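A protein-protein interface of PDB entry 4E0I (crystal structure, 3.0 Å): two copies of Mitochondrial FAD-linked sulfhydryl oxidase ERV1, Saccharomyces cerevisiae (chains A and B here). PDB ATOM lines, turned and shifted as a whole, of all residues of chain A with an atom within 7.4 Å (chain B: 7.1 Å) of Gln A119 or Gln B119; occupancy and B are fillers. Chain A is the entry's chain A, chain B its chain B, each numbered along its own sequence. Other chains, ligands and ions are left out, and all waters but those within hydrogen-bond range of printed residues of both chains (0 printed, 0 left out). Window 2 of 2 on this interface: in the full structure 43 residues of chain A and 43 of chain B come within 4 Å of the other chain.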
ATOM      1  N   GLN A 112     -20.223   6.116   5.861  1.00  0.00           N
ATOM      2  CA  GLN A 112     -20.178   4.693   6.197  1.00  0.00           C
ATOM      3  C   GLN A 112     -20.798   4.435   7.572  1.00  0.00           C
ATOM      4  O   GLN A 112     -21.588   3.504   7.737  1.00  0.00           O
ATOM      5  CB  GLN A 112     -18.738   4.171   6.160  1.00  0.00           C
ATOM      6  CG  GLN A 112     -18.613   2.664   6.344  1.00  0.00           C
ATOM      7  CD  GLN A 112     -17.200   2.217   6.672  1.00  0.00           C
ATOM      8  OE1 GLN A 112     -16.226   2.730   6.121  1.00  0.00           O
ATOM      9  NE2 GLN A 112     -17.084   1.245   7.570  1.00  0.00           N
ATOM     10  N   GLN A 113     -20.437   5.273   8.542  1.00  0.00           N
ATOM     11  CA  GLN A 113     -20.906   5.139   9.923  1.00  0.00           C
ATOM     12  C   GLN A 113     -22.404   5.388  10.065  1.00  0.00           C
ATOM     13  O   GLN A 113     -23.052   4.797  10.927  1.00  0.00           O
ATOM     14  CB  GLN A 113     -20.128   6.078  10.846  1.00  0.00           C
ATOM     15  CG  GLN A 113     -18.669   5.691  11.034  1.00  0.00           C
ATOM     16  CD  GLN A 113     -17.834   6.809  11.628  1.00  0.00           C
ATOM     17  OE1 GLN A 113     -18.030   7.984  11.314  1.00  0.00           O
ATOM     18  NE2 GLN A 113     -16.889   6.447  12.486  1.00  0.00           N
ATOM     19  N   LYS A 114     -22.942   6.268   9.221  1.00  0.00           N
ATOM     20  CA  LYS A 114     -24.380   6.525   9.174  1.00  0.00           C
ATOM     21  C   LYS A 114     -25.132   5.285   8.695  1.00  0.00           C
ATOM     22  O   LYS A 114     -26.078   4.837   9.345  1.00  0.00           O
ATOM     23  CB  LYS A 114     -24.694   7.708   8.254  1.00  0.00           C
ATOM     24  CG  LYS A 114     -24.304   9.068   8.808  1.00  0.00           C
ATOM     25  CD  LYS A 114     -24.652  10.169   7.819  1.00  0.00           C
ATOM     26  CE  LYS A 114     -24.290  11.540   8.363  1.00  0.00           C
ATOM     27  NZ  LYS A 114     -24.565  12.614   7.370  1.00  0.00           N
ATOM     28  N   GLY A 115     -24.693   4.740   7.563  1.00  0.00           N
ATOM     29  CA  GLY A 115     -25.312   3.561   6.963  1.00  0.00           C
ATOM     30  C   GLY A 115     -25.153   2.301   7.791  1.00  0.00           C
ATOM     31  O   GLY A 115     -26.087   1.504   7.894  1.00  0.00           O
ATOM     32  N   GLU A 116     -23.970   2.121   8.378  1.00  0.00           N
ATOM     33  CA  GLU A 116     -23.702   0.977   9.253  1.00  0.00           C
ATOM     34  C   GLU A 116     -24.543   1.028  10.524  1.00  0.00           C
ATOM     35  O   GLU A 116     -25.078   0.004  10.954  1.00  0.00           O
ATOM     36  CB  GLU A 116     -22.215   0.875   9.601  1.00  0.00           C
ATOM     37  CG  GLU A 116     -21.367   0.234   8.513  1.00  0.00           C
ATOM     38  CD  GLU A 116     -20.040  -0.297   9.027  1.00  0.00           C
ATOM     39  OE1 GLU A 116     -19.384   0.386   9.842  1.00  0.00           O
ATOM     40  OE2 GLU A 116     -19.650  -1.405   8.603  1.00  0.00           O
ATOM     41  N   MET A 117     -24.658   2.219  11.112  1.00  0.00           N
ATOM     42  CA  MET A 117     -25.500   2.432  12.290  1.00  0.00           C
ATOM     43  C   MET A 117     -26.956   2.077  11.994  1.00  0.00           C
ATOM     44  O   MET A 117     -27.616   1.431  12.808  1.00  0.00           O
ATOM     45  CB  MET A 117     -25.396   3.880  12.781  1.00  0.00           C
ATOM     46  CG  MET A 117     -26.174   4.181  14.058  1.00  0.00           C
ATOM     47  SD  MET A 117     -25.637   3.234  15.496  1.00  0.00           S
ATOM     48  CE  MET A 117     -23.956   3.830  15.685  1.00  0.00           C
ATOM     49  N   LYS A 118     -27.442   2.500  10.827  1.00  0.00           N
ATOM     50  CA  LYS A 118     -28.803   2.195  10.383  1.00  0.00           C
ATOM     51  C   LYS A 118     -29.044   0.692  10.282  1.00  0.00           C
ATOM     52  O   LYS A 118     -30.054   0.189  10.780  1.00  0.00           O
ATOM     53  CB  LYS A 118     -29.099   2.856   9.034  1.00  0.00           C
ATOM     54  CG  LYS A 118     -29.415   4.340   9.104  1.00  0.00           C
ATOM     55  CD  LYS A 118     -29.969   4.829   7.774  1.00  0.00           C
ATOM     56  CE  LYS A 118     -30.089   6.344   7.742  1.00  0.00           C
ATOM     57  NZ  LYS A 118     -30.698   6.817   6.467  1.00  0.00           N
ATOM     58  N   GLN A 119     -28.116  -0.012   9.635  1.00  0.00           N
ATOM     59  CA  GLN A 119     -28.189  -1.467   9.489  1.00  0.00           C
ATOM     60  C   GLN A 119     -28.147  -2.142  10.854  1.00  0.00           C
ATOM     61  O   GLN A 119     -28.956  -3.025  11.142  1.00  0.00           O
ATOM     62  CB  GLN A 119     -27.045  -1.991   8.617  1.00  0.00           C
ATOM     63  CG  GLN A 119     -27.119  -1.590   7.153  1.00  0.00           C
ATOM     64  CD  GLN A 119     -25.893  -2.019   6.369  1.00  0.00           C
ATOM     65  OE1 GLN A 119     -25.709  -3.200   6.077  1.00  0.00           O
ATOM     66  NE2 GLN A 119     -25.049  -1.054   6.017  1.00  0.00           N
ATOM     67  N   PHE A 120     -27.199  -1.707  11.683  1.00  0.00           N
ATOM     68  CA  PHE A 120     -27.027  -2.202  13.047  1.00  0.00           C
ATOM     69  C   PHE A 120     -28.354  -2.267  13.800  1.00  0.00           C
ATOM     70  O   PHE A 120     -28.676  -3.286  14.411  1.00  0.00           O
ATOM     71  CB  PHE A 120     -26.028  -1.317  13.801  1.00  0.00           C
ATOM     72  CG  PHE A 120     -25.713  -1.793  15.191  1.00  0.00           C
ATOM     73  CD1 PHE A 120     -24.966  -2.950  15.393  1.00  0.00           C
ATOM     74  CD2 PHE A 120     -26.148  -1.075  16.300  1.00  0.00           C
ATOM     75  CE1 PHE A 120     -24.671  -3.388  16.675  1.00  0.00           C
ATOM     76  CE2 PHE A 120     -25.854  -1.508  17.584  1.00  0.00           C
ATOM     77  CZ  PHE A 120     -25.116  -2.667  17.771  1.00  0.00           C
ATOM     78  N   LEU A 121     -29.117  -1.177  13.732  1.00  0.00           N
ATOM     79  CA  LEU A 121     -30.410  -1.075  14.406  1.00  0.00           C
ATOM     80  C   LEU A 121     -31.468  -1.981  13.779  1.00  0.00           C
ATOM     81  O   LEU A 121     -32.291  -2.560  14.493  1.00  0.00           O
ATOM     82  CB  LEU A 121     -30.889   0.382  14.433  1.00  0.00           C
ATOM     83  CG  LEU A 121     -29.963   1.407  15.101  1.00  0.00           C
ATOM     84  CD1 LEU A 121     -30.437   2.826  14.831  1.00  0.00           C
ATOM     85  CD2 LEU A 121     -29.828   1.165  16.600  1.00  0.00           C
ATOM     86  N   ASN A 122     -31.444  -2.098  12.452  1.00  0.00           N
ATOM     87  CA  ASN A 122     -32.342  -3.005  11.734  1.00  0.00           C
ATOM     88  C   ASN A 122     -32.076  -4.465  12.079  1.00  0.00           C
ATOM     89  O   ASN A 122     -32.990  -5.187  12.478  1.00  0.00           O
ATOM     90  CB  ASN A 122     -32.245  -2.795  10.219  1.00  0.00           C
ATOM     91  CG  ASN A 122     -33.161  -1.693   9.719  1.00  0.00           C
ATOM     92  OD1 ASN A 122     -34.304  -1.565  10.162  1.00  0.00           O
ATOM     93  ND2 ASN A 122     -32.665  -0.897   8.780  1.00  0.00           N
ATOM     94  N   ILE A 123     -30.821  -4.885  11.930  1.00  0.00           N
ATOM     95  CA  ILE A 123     -30.409  -6.246  12.274  1.00  0.00           C
ATOM     96  C   ILE A 123     -30.767  -6.543  13.731  1.00  0.00           C
ATOM     97  O   ILE A 123     -31.317  -7.603  14.032  1.00  0.00           O
ATOM     98  CB  ILE A 123     -28.904  -6.483  12.009  1.00  0.00           C
ATOM     99  CG1 ILE A 123     -28.575  -6.208  10.537  1.00  0.00           C
ATOM    100  CG2 ILE A 123     -28.517  -7.911  12.368  1.00  0.00           C
ATOM    101  CD1 ILE A 123     -27.119  -5.883  10.269  1.00  0.00           C
ATOM    102  N   PHE A 124     -30.483  -5.585  14.614  1.00  0.00           N
ATOM    103  CA  PHE A 124     -30.854  -5.673  16.027  1.00  0.00           C
ATOM    104  C   PHE A 124     -32.347  -5.944  16.213  1.00  0.00           C
ATOM    105  O   PHE A 124     -32.728  -6.827  16.983  1.00  0.00           O
ATOM    106  CB  PHE A 124     -30.460  -4.389  16.765  1.00  0.00           C
ATOM    107  CG  PHE A 124     -30.457  -4.522  18.261  1.00  0.00           C
ATOM    108  CD1 PHE A 124     -29.341  -5.023  18.922  1.00  0.00           C
ATOM    109  CD2 PHE A 124     -31.564  -4.140  19.011  1.00  0.00           C
ATOM    110  CE1 PHE A 124     -29.332  -5.147  20.302  1.00  0.00           C
ATOM    111  CE2 PHE A 124     -31.560  -4.261  20.392  1.00  0.00           C
ATOM    112  CZ  PHE A 124     -30.442  -4.765  21.038  1.00  0.00           C
ATOM    113  N   SER A 125     -33.182  -5.190  15.496  1.00  0.00           N
ATOM    114  CA  SER A 125     -34.638  -5.330  15.580  1.00  0.00           C
ATOM    115  C   SER A 125     -35.140  -6.691  15.085  1.00  0.00           C
ATOM    116  O   SER A 125     -36.255  -7.102  15.414  1.00  0.00           O
ATOM    117  CB  SER A 125     -35.341  -4.193  14.830  1.00  0.00           C
ATOM    118  OG  SER A 125     -35.091  -4.254  13.438  1.00  0.00           O
ATOM    119  N   HIS A 126     -34.316  -7.381  14.297  1.00  0.00           N
ATOM    120  CA  HIS A 126     -34.632  -8.732  13.838  1.00  0.00           C
ATOM    121  C   HIS A 126     -34.169  -9.771  14.818  1.00  0.00           C
ATOM    122  O   HIS A 126     -34.944 -10.643  15.219  1.00  0.00           O
ATOM    123  CB  HIS A 126     -34.010  -9.017  12.472  1.00  0.00           C
ATOM    124  CG  HIS A 126     -34.427  -8.054  11.385  1.00  0.00           C
ATOM    125  ND1 HIS A 126     -35.713  -7.732  11.153  1.00  0.00           N
ATOM    126  CD2 HIS A 126     -33.672  -7.364  10.438  1.00  0.00           C
ATOM    127  CE1 HIS A 126     -35.779  -6.866  10.124  1.00  0.00           C
ATOM    128  NE2 HIS A 126     -34.529  -6.643   9.687  1.00  0.00           N
ATOM    129  N   GLN B 112     -30.677 -15.013   4.803  1.00  0.00           N
ATOM    130  CA  GLN B 112     -30.824 -13.662   5.342  1.00  0.00           C
ATOM    131  C   GLN B 112     -30.311 -13.573   6.780  1.00  0.00           C
ATOM    132  O   GLN B 112     -29.625 -12.616   7.140  1.00  0.00           O
ATOM    133  CB  GLN B 112     -32.286 -13.204   5.259  1.00  0.00           C
ATOM    134  CG  GLN B 112     -32.526 -11.734   5.590  1.00  0.00           C
ATOM    135  CD  GLN B 112     -31.879 -10.766   4.607  1.00  0.00           C
ATOM    136  OE1 GLN B 112     -31.617  -9.611   4.947  1.00  0.00           O
ATOM    137  NE2 GLN B 112     -31.622 -11.228   3.386  1.00  0.00           N
ATOM    138  N   GLN B 113     -30.645 -14.580   7.587  1.00  0.00           N
ATOM    139  CA  GLN B 113     -30.202 -14.649   8.979  1.00  0.00           C
ATOM    140  C   GLN B 113     -28.699 -14.893   9.081  1.00  0.00           C
ATOM    141  O   GLN B 113     -28.038 -14.353   9.969  1.00  0.00           O
ATOM    142  CB  GLN B 113     -30.965 -15.737   9.735  1.00  0.00           C
ATOM    143  CG  GLN B 113     -32.420 -15.392  10.011  1.00  0.00           C
ATOM    144  CD  GLN B 113     -33.200 -16.549  10.604  1.00  0.00           C
ATOM    145  OE1 GLN B 113     -32.979 -17.710  10.258  1.00  0.00           O
ATOM    146  NE2 GLN B 113     -34.129 -16.234  11.497  1.00  0.00           N
ATOM    147  N   LYS B 114     -28.175 -15.709   8.169  1.00  0.00           N
ATOM    148  CA  LYS B 114     -26.741 -15.988   8.086  1.00  0.00           C
ATOM    149  C   LYS B 114     -25.962 -14.751   7.648  1.00  0.00           C
ATOM    150  O   LYS B 114     -24.863 -14.493   8.146  1.00  0.00           O
ATOM    151  CB  LYS B 114     -26.477 -17.145   7.121  1.00  0.00           C
ATOM    152  CG  LYS B 114     -26.840 -18.513   7.680  1.00  0.00           C
ATOM    153  CD  LYS B 114     -27.213 -19.499   6.581  1.00  0.00           C
ATOM    154  CE  LYS B 114     -25.992 -20.053   5.861  1.00  0.00           C
ATOM    155  NZ  LYS B 114     -26.384 -20.955   4.743  1.00  0.00           N
ATOM    156  N   GLY B 115     -26.541 -13.995   6.717  1.00  0.00           N
ATOM    157  CA  GLY B 115     -25.946 -12.754   6.233  1.00  0.00           C
ATOM    158  C   GLY B 115     -25.933 -11.667   7.290  1.00  0.00           C
ATOM    159  O   GLY B 115     -24.909 -11.017   7.506  1.00  0.00           O
ATOM    160  N   GLU B 116     -27.073 -11.483   7.955  1.00  0.00           N
ATOM    161  CA  GLU B 116     -27.222 -10.456   8.988  1.00  0.00           C
ATOM    162  C   GLU B 116     -26.381 -10.726  10.233  1.00  0.00           C
ATOM    163  O   GLU B 116     -25.930  -9.786  10.888  1.00  0.00           O
ATOM    164  CB  GLU B 116     -28.691 -10.281   9.371  1.00  0.00           C
ATOM    165  CG  GLU B 116     -29.498  -9.475   8.365  1.00  0.00           C
ATOM    166  CD  GLU B 116     -30.995  -9.578   8.589  1.00  0.00           C
ATOM    167  OE1 GLU B 116     -31.460 -10.612   9.118  1.00  0.00           O
ATOM    168  OE2 GLU B 116     -31.714  -8.623   8.227  1.00  0.00           O
ATOM    169  N   MET B 117     -26.179 -12.002  10.556  1.00  0.00           N
ATOM    170  CA  MET B 117     -25.335 -12.382  11.687  1.00  0.00           C
ATOM    171  C   MET B 117     -23.877 -12.010  11.426  1.00  0.00           C
ATOM    172  O   MET B 117     -23.181 -11.540  12.328  1.00  0.00           O
ATOM    173  CB  MET B 117     -25.468 -13.876  12.000  1.00  0.00           C
ATOM    174  CG  MET B 117     -24.824 -14.306  13.313  1.00  0.00           C
ATOM    175  SD  MET B 117     -25.197 -13.238  14.722  1.00  0.00           S
ATOM    176  CE  MET B 117     -26.967 -13.462  14.875  1.00  0.00           C
ATOM    177  N   LYS B 118     -23.431 -12.222  10.188  1.00  0.00           N
ATOM    178  CA  LYS B 118     -22.103 -11.801   9.751  1.00  0.00           C
ATOM    179  C   LYS B 118     -21.972 -10.280   9.793  1.00  0.00           C
ATOM    180  O   LYS B 118     -20.964  -9.754  10.268  1.00  0.00           O
ATOM    181  CB  LYS B 118     -21.807 -12.310   8.337  1.00  0.00           C
ATOM    182  CG  LYS B 118     -21.467 -13.791   8.247  1.00  0.00           C
ATOM    183  CD  LYS B 118     -21.078 -14.171   6.826  1.00  0.00           C
ATOM    184  CE  LYS B 118     -20.639 -15.623   6.735  1.00  0.00           C
ATOM    185  NZ  LYS B 118     -20.245 -16.000   5.348  1.00  0.00           N
ATOM    186  N   GLN B 119     -22.998  -9.586   9.300  1.00  0.00           N
ATOM    187  CA  GLN B 119     -23.024  -8.121   9.267  1.00  0.00           C
ATOM    188  C   GLN B 119     -23.000  -7.517  10.667  1.00  0.00           C
ATOM    189  O   GLN B 119     -22.169  -6.655  10.962  1.00  0.00           O
ATOM    190  CB  GLN B 119     -24.264  -7.613   8.526  1.00  0.00           C
ATOM    191  CG  GLN B 119     -24.261  -7.842   7.026  1.00  0.00           C
ATOM    192  CD  GLN B 119     -25.403  -7.118   6.342  1.00  0.00           C
ATOM    193  OE1 GLN B 119     -26.484  -7.675   6.157  1.00  0.00           O
ATOM    194  NE2 GLN B 119     -25.173  -5.861   5.981  1.00  0.00           N
ATOM    195  N   PHE B 120     -23.920  -7.978  11.515  1.00  0.00           N
ATOM    196  CA  PHE B 120     -24.054  -7.506  12.893  1.00  0.00           C
ATOM    197  C   PHE B 120     -22.719  -7.525  13.628  1.00  0.00           C
ATOM    198  O   PHE B 120     -22.371  -6.564  14.313  1.00  0.00           O
ATOM    199  CB  PHE B 120     -25.087  -8.357  13.643  1.00  0.00           C
ATOM    200  CG  PHE B 120     -25.443  -7.833  15.007  1.00  0.00           C
ATOM    201  CD1 PHE B 120     -26.348  -6.786  15.152  1.00  0.00           C
ATOM    202  CD2 PHE B 120     -24.889  -8.401  16.150  1.00  0.00           C
ATOM    203  CE1 PHE B 120     -26.683  -6.306  16.410  1.00  0.00           C
ATOM    204  CE2 PHE B 120     -25.220  -7.925  17.411  1.00  0.00           C
ATOM    205  CZ  PHE B 120     -26.118  -6.877  17.540  1.00  0.00           C
ATOM    206  N   LEU B 121     -21.975  -8.618  13.469  1.00  0.00           N
ATOM    207  CA  LEU B 121     -20.681  -8.786  14.125  1.00  0.00           C
ATOM    208  C   LEU B 121     -19.580  -7.936  13.489  1.00  0.00           C
ATOM    209  O   LEU B 121     -18.674  -7.473  14.186  1.00  0.00           O
ATOM    210  CB  LEU B 121     -20.276 -10.264  14.160  1.00  0.00           C
ATOM    211  CG  LEU B 121     -21.133 -11.202  15.020  1.00  0.00           C
ATOM    212  CD1 LEU B 121     -20.854 -12.654  14.667  1.00  0.00           C
ATOM    213  CD2 LEU B 121     -20.924 -10.960  16.508  1.00  0.00           C
ATOM    214  N   ASN B 122     -19.660  -7.739  12.173  1.00  0.00           N
ATOM    215  CA  ASN B 122     -18.737  -6.851  11.461  1.00  0.00           C
ATOM    216  C   ASN B 122     -18.926  -5.395  11.875  1.00  0.00           C
ATOM    217  O   ASN B 122     -17.951  -4.685  12.128  1.00  0.00           O
ATOM    218  CB  ASN B 122     -18.901  -6.989   9.944  1.00  0.00           C
ATOM    219  CG  ASN B 122     -18.366  -8.306   9.409  1.00  0.00           C
ATOM    220  OD1 ASN B 122     -17.668  -9.045  10.107  1.00  0.00           O
ATOM    221  ND2 ASN B 122     -18.694  -8.606   8.158  1.00  0.00           N
ATOM    222  N   ILE B 123     -20.186  -4.966  11.940  1.00  0.00           N
ATOM    223  CA  ILE B 123     -20.538  -3.621  12.393  1.00  0.00           C
ATOM    224  C   ILE B 123     -20.186  -3.450  13.872  1.00  0.00           C
ATOM    225  O   ILE B 123     -19.674  -2.403  14.273  1.00  0.00           O
ATOM    226  CB  ILE B 123     -22.034  -3.302  12.143  1.00  0.00           C
ATOM    227  CG1 ILE B 123     -22.335  -3.297  10.639  1.00  0.00           C
ATOM    228  CG2 ILE B 123     -22.417  -1.958  12.757  1.00  0.00           C
ATOM    229  CD1 ILE B 123     -23.807  -3.385  10.291  1.00  0.00           C
ATOM    230  N   PHE B 124     -20.444  -4.490  14.666  1.00  0.00           N
ATOM    231  CA  PHE B 124     -20.149  -4.485  16.102  1.00  0.00           C
ATOM    232  C   PHE B 124     -18.684  -4.167  16.394  1.00  0.00           C
ATOM    233  O   PHE B 124     -18.378  -3.412  17.319  1.00  0.00           O
ATOM    234  CB  PHE B 124     -20.527  -5.829  16.733  1.00  0.00           C
ATOM    235  CG  PHE B 124     -20.362  -5.867  18.225  1.00  0.00           C
ATOM    236  CD1 PHE B 124     -21.308  -5.277  19.058  1.00  0.00           C
ATOM    237  CD2 PHE B 124     -19.263  -6.496  18.802  1.00  0.00           C
ATOM    238  CE1 PHE B 124     -21.159  -5.309  20.436  1.00  0.00           C
ATOM    239  CE2 PHE B 124     -19.109  -6.532  20.180  1.00  0.00           C
ATOM    240  CZ  PHE B 124     -20.059  -5.939  20.998  1.00  0.00           C
ATOM    241  N   SER B 125     -17.790  -4.750  15.598  1.00  0.00           N
ATOM    242  CA  SER B 125     -16.354  -4.543  15.750  1.00  0.00           C
ATOM    243  C   SER B 125     -15.908  -3.151  15.291  1.00  0.00           C
ATOM    244  O   SER B 125     -14.774  -2.743  15.549  1.00  0.00           O
ATOM    245  CB  SER B 125     -15.580  -5.628  14.998  1.00  0.00           C
ATOM    246  OG  SER B 125     -15.917  -5.642  13.621  1.00  0.00           O
ATOM    247  N   HIS B 126     -16.798  -2.433  14.609  1.00  0.00           N
ATOM    248  CA  HIS B 126     -16.514  -1.067  14.170  1.00  0.00           C
ATOM    249  C   HIS B 126     -16.917  -0.034  15.188  1.00  0.00           C
ATOM    250  O   HIS B 126     -16.235   0.981  15.345  1.00  0.00           O
ATOM    251  CB  HIS B 126     -17.195  -0.756  12.837  1.00  0.00           C
ATOM    252  CG  HIS B 126     -16.665  -1.553  11.664  1.00  0.00           C
ATOM    253  ND1 HIS B 126     -15.366  -1.884  11.535  1.00  0.00           N
ATOM    254  CD2 HIS B 126     -17.310  -2.051  10.534  1.00  0.00           C
ATOM    255  CE1 HIS B 126     -15.192  -2.577  10.394  1.00  0.00           C
ATOM    256  NE2 HIS B 126     -16.382  -2.676   9.782  1.00  0.00           N
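OE1 of Gln A119 is in hydrogen-bond range of NE2 of Gln B119 (2.7 Å).
The side-chain amide nitrogen (NE2) of Gln A112 is in hydrogen-bond range of the side-chain carboxylate (OE1) of Glu A116 (3.3 Å).
The backbone carbonyl oxygen of Gly A115 lies within hydrogen-bond range of the side-chain amide nitrogen of Gln A119.
The side-chain amide oxygen of Gln B112 sits close to the side-chain carboxylate of Glu B116 (3.4 Å).
The backbone carbonyl oxygen (O) of Asn B122 lies close to a ring nitrogen (NE2) of His B126 (3.5 Å).
Glu A116 touches Ile B123 (O to CD1, 3.7 Å).
OE2 of Glu A116 touches CD2 of His B126 (3.1 Å).
CD1 of Ile B123 touches CB of Gln A119, at 3.9 Å.
CE1 of Phe B120 touches CE1 of Phe A120, at 3.6 Å.
CG2 of Ile B123 touches CD1 of Phe A120 (3.8 Å).
Ile A123 touches Glu B116.
Gln B119 touches Ile A123.
Ile A123 touches Phe B120.
CD1 of Phe A124 touches CE1 of Phe B120, 3.9 Å away.
CD2 of His A126 touches OE2 of Glu B116, 3.2 Å away.
Of chain B, only Gln B119 and Ile B123 come within 4 Å of Gln A119.
Gln B119 touches two residues of chain A.
Printed residues of chain A within 4 Å of His B126: Glu A116.
Of the printed residues of chain B, Phe A124 touches Phe B120 (3.9 Å).
Printed residues of chain A within 4 Å of Ile B123: Glu A116 (3.7 Å), Gln A119 (3.9 Å) and Phe A120 (3.8 Å).
Printed residues of chain A within 4 Å of Phe B120: Phe A120, Ile A123 and Phe A124.
Of the printed residues of chain B, His A126 touches Glu B116 (3.2 Å).
Hydrophobic or aromatic side chains of chain B within 4 Å of the printed part of chain A: Phe B120, Ile B123 and His B126.
Hydrophobic or aromatic side chains of chain A within 4 Å of the printed part of chain B: Phe A120, Ile A123, Phe A124 and His A126.
Among the printed residues, 11 pairs touch across the chains.
Among the printed residues, no Asp or Glu carboxylate lies within 4 Å of a Lys or Arg side-chain nitrogen of the other chain.
Glu A116 touches Ile B123, and with the chains exchanged Ile A123 touches Glu B116.
Gln A119 touches its own counterpart, Gln B119.
Gln A119 touches Ile B123, and with the chains exchanged Ile A123 touches Gln B119.
Phe A124 touches Phe B120, but with the chains exchanged Phe A120 does not touch Phe B124 (4.5 Å).
Positions printed for both chains: 112, 113, 114, 115, 116, 117, 118, 119, 120, 121, 122, 123, 124, 125 and 126.
Of the 11 pairs that touch across the chains among the printed residues, 10 have their exchanged pair printed and touching as well.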
